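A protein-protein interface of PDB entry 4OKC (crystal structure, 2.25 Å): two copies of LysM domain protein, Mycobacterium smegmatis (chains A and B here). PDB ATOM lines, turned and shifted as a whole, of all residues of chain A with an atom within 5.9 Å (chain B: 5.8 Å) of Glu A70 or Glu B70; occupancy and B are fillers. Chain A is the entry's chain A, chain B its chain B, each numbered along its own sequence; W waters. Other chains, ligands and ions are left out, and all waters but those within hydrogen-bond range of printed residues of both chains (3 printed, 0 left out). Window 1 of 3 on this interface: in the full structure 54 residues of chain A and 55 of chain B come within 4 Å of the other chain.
OE2 of Glu A70 lies within salt-bridge range of NH1 of Arg B55, at 2.7 Å. The backbone carbonyl oxygen (O) of Lys A71 lies within hydrogen-bond range of the backbone NH (N) of Thr B68 (2.9 Å). The backbone NH (N) of Thr A68 lies within hydrogen-bond range of the backbone carbonyl oxygen (O) of Lys B71, 2.8 Å away. The side-chain carboxylate of Glu B70 lies within salt-bridge range of the guanidinium group of Arg A55 (2.6 Å).
Val A54 touches Glu B70, and with the chains exchanged Glu A70 touches Val B54. Tyr A67 touches Lys B71, and with the chains exchanged Lys A71 touches Tyr B67. Thr A68 touches Glu B70, and with the chains exchanged Glu A70 touches Thr B68. Glu A70 touches its own counterpart, Glu B70. 8 positions are printed for both chains.
The backbone NH of Val B54 is in hydrogen-bond range of the backbone carbonyl oxygen of Tyr B67. O of Arg A55 is in hydrogen-bond range of N of Tyr A67, 2.9 Å away. The backbone carbonyl oxygen of Arg B55 is in hydrogen-bond range of the backbone NH of Tyr B67, 3.0 Å away. The backbone carbonyl oxygen (O) of Tyr A67 is in hydrogen-bond range of the backbone NH (N) of Val A54 (2.8 Å).
Of the printed residues of chain B, Arg A55 touches Glu B70 (2.6 Å). Ala A69 touches none of the printed residues of chain B. Glu A70 touches five residues of chain B. Of the printed residues of chain B, Pro A72 touches Tyr B67 (3.6 Å). Ala B69 touches none of the printed residues of chain A. Of chain A, only Val A54 (3.4 Å), Arg A55 (2.6 Å), Tyr A67 (3.5 Å), Thr A68 (3.1 Å) and Glu A70 (3.7 Å) come within 4 Å of Glu B70. The nearest residue of chain A that does not touch Glu B70 is Ala A69 (4.1 Å). The nearest printed residue of chain A that does not touch Thr B68 is Pro A72 (5.1 Å).
Of the 8 printed residues of chain A, 7 touch a printed residue of chain B. Hydrophobic or aromatic side chains of chain A that line the printed part of chain B: Val A54, Tyr A67 and Pro A72.
Among the printed residues, pairs that only touch across the chains: Val A54 with Glu B70 (3.4 Å), Tyr A67 with Glu B70 (3.5 Å), Tyr A67 with Lys B71 (3.1 Å), Tyr A67 with Pro B72 (3.8 Å), Thr A68 with Glu B70 (3.1 Å), Glu A70 with Val B54 (2.9 Å), Glu A70 with Tyr B67 (3.4 Å), Glu A70 with Thr B68 (3.2 Å), Glu A70 with Glu B70 (3.7 Å), Lys A71 with Tyr B67 (3.4 Å) and Pro A72 with Tyr B67 (3.6 Å).
Water W1 bridges OE1 of Glu A70 (2.5 Å) and N of Glu B70 (3.3 Å). Water W3 bridges OE1 of Glu A70 (2.6 Å) and NH1 of Arg B55 (2.9 Å). Water W2 lies within hydrogen-bond range of the backbone NH of Lys A71 (2.8 Å), the backbone carbonyl oxygen of Ala B69 (2.9 Å) and the backbone carbonyl oxygen of Thr B68 (2.9 Å).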
ATOM      1  N   VAL A  54      16.852  16.099  25.424  1.00  0.00           N
ATOM      2  CA  VAL A  54      17.680  15.432  26.427  1.00  0.00           C
ATOM      3  C   VAL A  54      16.816  14.801  27.516  1.00  0.00           C
ATOM      4  O   VAL A  54      17.184  13.771  28.107  1.00  0.00           O
ATOM      5  CB  VAL A  54      18.748  16.362  27.121  1.00  0.00           C
ATOM      6  CG1 VAL A  54      18.124  17.589  27.814  1.00  0.00           C
ATOM      7  CG2 VAL A  54      19.534  15.566  28.180  1.00  0.00           C
ATOM      8  N   ARG A  55      15.672  15.418  27.783  1.00  0.00           N
ATOM      9  CA  ARG A  55      14.797  14.971  28.842  1.00  0.00           C
ATOM     10  C   ARG A  55      13.336  15.417  28.671  1.00  0.00           C
ATOM     11  O   ARG A  55      13.029  16.477  28.141  1.00  0.00           O
ATOM     12  CB  ARG A  55      15.342  15.369  30.212  1.00  0.00           C
ATOM     13  CG  ARG A  55      15.255  16.890  30.527  1.00  0.00           C
ATOM     14  CD  ARG A  55      15.597  17.167  32.000  1.00  0.00           C
ATOM     15  NE  ARG A  55      15.400  18.579  32.388  1.00  0.00           N
ATOM     16  CZ  ARG A  55      16.113  19.594  31.897  1.00  0.00           C
ATOM     17  NH1 ARG A  55      17.028  19.353  30.960  1.00  0.00           N
ATOM     18  NH2 ARG A  55      15.894  20.844  32.291  1.00  0.00           N
ATOM     19  N   TYR A  67      13.195  19.215  27.143  1.00  0.00           N
ATOM     20  CA  TYR A  67      14.246  20.190  26.955  1.00  0.00           C
ATOM     21  C   TYR A  67      15.207  19.710  25.900  1.00  0.00           C
ATOM     22  O   TYR A  67      15.613  18.529  25.902  1.00  0.00           O
ATOM     23  CB  TYR A  67      14.983  20.403  28.265  1.00  0.00           C
ATOM     24  CG  TYR A  67      14.154  21.142  29.304  1.00  0.00           C
ATOM     25  CD1 TYR A  67      14.008  22.519  29.249  1.00  0.00           C
ATOM     26  CD2 TYR A  67      13.532  20.447  30.351  1.00  0.00           C
ATOM     27  CE1 TYR A  67      13.262  23.206  30.218  1.00  0.00           C
ATOM     28  CE2 TYR A  67      12.779  21.118  31.319  1.00  0.00           C
ATOM     29  CZ  TYR A  67      12.652  22.505  31.246  1.00  0.00           C
ATOM     30  OH  TYR A  67      11.909  23.179  32.195  1.00  0.00           O
ATOM     31  N   THR A  68      15.580  20.634  25.013  1.00  0.00           N
ATOM     32  CA  THR A  68      16.687  20.396  24.089  1.00  0.00           C
ATOM     33  C   THR A  68      18.031  20.676  24.777  1.00  0.00           C
ATOM     34  O   THR A  68      18.071  21.474  25.707  1.00  0.00           O
ATOM     35  CB  THR A  68      16.540  21.173  22.771  1.00  0.00           C
ATOM     36  OG1 THR A  68      16.597  22.588  23.013  1.00  0.00           O
ATOM     37  CG2 THR A  68      15.263  20.803  22.115  1.00  0.00           C
ATOM     38  N   ALA A  69      19.091  19.985  24.355  1.00  0.00           N
ATOM     39  CA  ALA A  69      20.453  20.185  24.854  1.00  0.00           C
ATOM     40  C   ALA A  69      20.895  21.653  24.737  1.00  0.00           C
ATOM     41  O   ALA A  69      20.453  22.387  23.841  1.00  0.00           O
ATOM     42  CB  ALA A  69      21.430  19.317  24.074  1.00  0.00           C
ATOM     43  N   GLU A  70      21.787  22.054  25.627  1.00  0.00           N
ATOM     44  CA  GLU A  70      22.385  23.362  25.598  1.00  0.00           C
ATOM     45  C   GLU A  70      23.068  23.589  24.260  1.00  0.00           C
ATOM     46  O   GLU A  70      23.862  22.752  23.830  1.00  0.00           O
ATOM     47  CB  GLU A  70      23.403  23.442  26.727  1.00  0.00           C
ATOM     48  CG  GLU A  70      22.807  23.538  28.116  1.00  0.00           C
ATOM     49  CD  GLU A  70      23.829  23.975  29.156  1.00  0.00           C
ATOM     50  OE1 GLU A  70      23.552  23.790  30.360  1.00  0.00           O
ATOM     51  OE2 GLU A  70      24.906  24.519  28.786  1.00  0.00           O
ATOM     52  N   LYS A  71      22.723  24.689  23.579  1.00  0.00           N
ATOM     53  CA  LYS A  71      23.288  25.018  22.255  1.00  0.00           C
ATOM     54  C   LYS A  71      24.306  26.157  22.358  1.00  0.00           C
ATOM     55  O   LYS A  71      24.168  27.039  23.236  1.00  0.00           O
ATOM     56  CB  LYS A  71      22.199  25.488  21.304  1.00  0.00           C
ATOM     57  CG  LYS A  71      21.299  24.402  20.707  1.00  0.00           C
ATOM     58  CD  LYS A  71      19.834  24.911  20.683  1.00  0.00           C
ATOM     59  CE  LYS A  71      19.603  26.140  19.778  1.00  0.00           C
ATOM     60  NZ  LYS A  71      20.106  25.936  18.359  1.00  0.00           N
ATOM     61  N   PRO A  72      25.289  26.175  21.423  1.00  0.00           N
ATOM     62  CA  PRO A  72      26.356  27.164  21.345  1.00  0.00           C
ATOM     63  C   PRO A  72      25.925  28.408  20.587  1.00  0.00           C
ATOM     64  O   PRO A  72      25.564  28.311  19.420  1.00  0.00           O
ATOM     65  CB  PRO A  72      27.481  26.425  20.570  1.00  0.00           C
ATOM     66  CG  PRO A  72      26.828  25.243  19.880  1.00  0.00           C
ATOM     67  CD  PRO A  72      25.359  25.221  20.290  1.00  0.00           C
ATOM     68  N   VAL B  54      24.957  30.011  30.044  1.00  0.00           N
ATOM     69  CA  VAL B  54      25.242  29.347  31.313  1.00  0.00           C
ATOM     70  C   VAL B  54      26.758  29.179  31.587  1.00  0.00           C
ATOM     71  O   VAL B  54      27.186  29.200  32.712  1.00  0.00           O
ATOM     72  CB  VAL B  54      24.483  27.995  31.486  1.00  0.00           C
ATOM     73  CG1 VAL B  54      24.760  27.000  30.318  1.00  0.00           C
ATOM     74  CG2 VAL B  54      24.899  27.329  32.843  1.00  0.00           C
ATOM     75  N   ARG B  55      27.559  29.065  30.538  1.00  0.00           N
ATOM     76  CA  ARG B  55      28.972  28.881  30.694  1.00  0.00           C
ATOM     77  C   ARG B  55      29.722  29.234  29.419  1.00  0.00           C
ATOM     78  O   ARG B  55      29.175  29.169  28.316  1.00  0.00           O
ATOM     79  CB  ARG B  55      29.272  27.426  31.090  1.00  0.00           C
ATOM     80  CG  ARG B  55      28.953  26.405  29.990  1.00  0.00           C
ATOM     81  CD  ARG B  55      29.763  25.119  30.178  1.00  0.00           C
ATOM     82  NE  ARG B  55      29.592  24.177  29.063  1.00  0.00           N
ATOM     83  CZ  ARG B  55      28.440  23.582  28.776  1.00  0.00           C
ATOM     84  NH1 ARG B  55      27.374  23.875  29.515  1.00  0.00           N
ATOM     85  NH2 ARG B  55      28.334  22.716  27.767  1.00  0.00           N
ATOM     86  N   TYR B  67      27.579  28.580  25.867  1.00  0.00           N
ATOM     87  CA  TYR B  67      26.356  27.753  25.770  1.00  0.00           C
ATOM     88  C   TYR B  67      25.195  28.438  26.443  1.00  0.00           C
ATOM     89  O   TYR B  67      25.374  29.089  27.480  1.00  0.00           O
ATOM     90  CB  TYR B  67      26.561  26.371  26.418  1.00  0.00           C
ATOM     91  CG  TYR B  67      27.383  25.467  25.527  1.00  0.00           C
ATOM     92  CD1 TYR B  67      26.823  24.882  24.404  1.00  0.00           C
ATOM     93  CD2 TYR B  67      28.750  25.288  25.744  1.00  0.00           C
ATOM     94  CE1 TYR B  67      27.593  24.127  23.537  1.00  0.00           C
ATOM     95  CE2 TYR B  67      29.509  24.507  24.911  1.00  0.00           C
ATOM     96  CZ  TYR B  67      28.914  23.925  23.810  1.00  0.00           C
ATOM     97  OH  TYR B  67      29.659  23.173  22.937  1.00  0.00           O
ATOM     98  N   THR B  68      24.009  28.298  25.857  1.00  0.00           N
ATOM     99  CA  THR B  68      22.790  28.769  26.504  1.00  0.00           C
ATOM    100  C   THR B  68      22.071  27.581  27.150  1.00  0.00           C
ATOM    101  O   THR B  68      22.220  26.460  26.692  1.00  0.00           O
ATOM    102  CB  THR B  68      21.847  29.419  25.503  1.00  0.00           C
ATOM    103  OG1 THR B  68      21.729  28.548  24.384  1.00  0.00           O
ATOM    104  CG2 THR B  68      22.388  30.723  25.051  1.00  0.00           C
ATOM    105  N   ALA B  69      21.312  27.855  28.209  1.00  0.00           N
ATOM    106  CA  ALA B  69      20.544  26.869  28.942  1.00  0.00           C
ATOM    107  C   ALA B  69      19.539  26.059  28.063  1.00  0.00           C
ATOM    108  O   ALA B  69      19.050  26.542  27.043  1.00  0.00           O
ATOM    109  CB  ALA B  69      19.822  27.559  30.096  1.00  0.00           C
ATOM    110  N   GLU B  70      19.237  24.843  28.491  1.00  0.00           N
ATOM    111  CA  GLU B  70      18.335  23.945  27.797  1.00  0.00           C
ATOM    112  C   GLU B  70      16.982  24.567  27.574  1.00  0.00           C
ATOM    113  O   GLU B  70      16.351  25.071  28.512  1.00  0.00           O
ATOM    114  CB  GLU B  70      18.204  22.647  28.598  1.00  0.00           C
ATOM    115  CG  GLU B  70      19.495  21.858  28.607  1.00  0.00           C
ATOM    116  CD  GLU B  70      19.521  20.811  29.688  1.00  0.00           C
ATOM    117  OE1 GLU B  70      18.953  21.062  30.768  1.00  0.00           O
ATOM    118  OE2 GLU B  70      20.125  19.754  29.469  1.00  0.00           O
ATOM    119  N   LYS B  71      16.558  24.541  26.318  1.00  0.00           N
ATOM    120  CA  LYS B  71      15.340  25.198  25.863  1.00  0.00           C
ATOM    121  C   LYS B  71      14.123  24.229  25.935  1.00  0.00           C
ATOM    122  O   LYS B  71      14.247  23.035  25.636  1.00  0.00           O
ATOM    123  CB  LYS B  71      15.561  25.694  24.416  1.00  0.00           C
ATOM    124  CG  LYS B  71      14.407  26.562  23.826  1.00  0.00           C
ATOM    125  CD  LYS B  71      14.664  27.037  22.380  1.00  0.00           C
ATOM    126  CE  LYS B  71      13.489  27.891  21.863  1.00  0.00           C
ATOM    127  NZ  LYS B  71      13.742  28.346  20.451  1.00  0.00           N
ATOM    128  N   PRO B  72      12.947  24.748  26.337  1.00  0.00           N
ATOM    129  CA  PRO B  72      11.680  24.016  26.268  1.00  0.00           C
ATOM    130  C   PRO B  72      11.135  23.905  24.844  1.00  0.00           C
ATOM    131  O   PRO B  72      11.080  24.904  24.117  1.00  0.00           O
ATOM    132  CB  PRO B  72      10.712  24.888  27.112  1.00  0.00           C
ATOM    133  CG  PRO B  72      11.625  25.769  27.945  1.00  0.00           C
ATOM    134  CD  PRO B  72      12.785  26.041  27.020  1.00  0.00           C
HETATM  135  O   HOH W   1      21.169  24.139  31.028  1.00  0.00           O
HETATM  136  O   HOH W   2      20.336  25.859  24.544  1.00  0.00           O
HETATM  137  O   HOH W   3      25.607  24.439  31.733  1.00  0.00           O
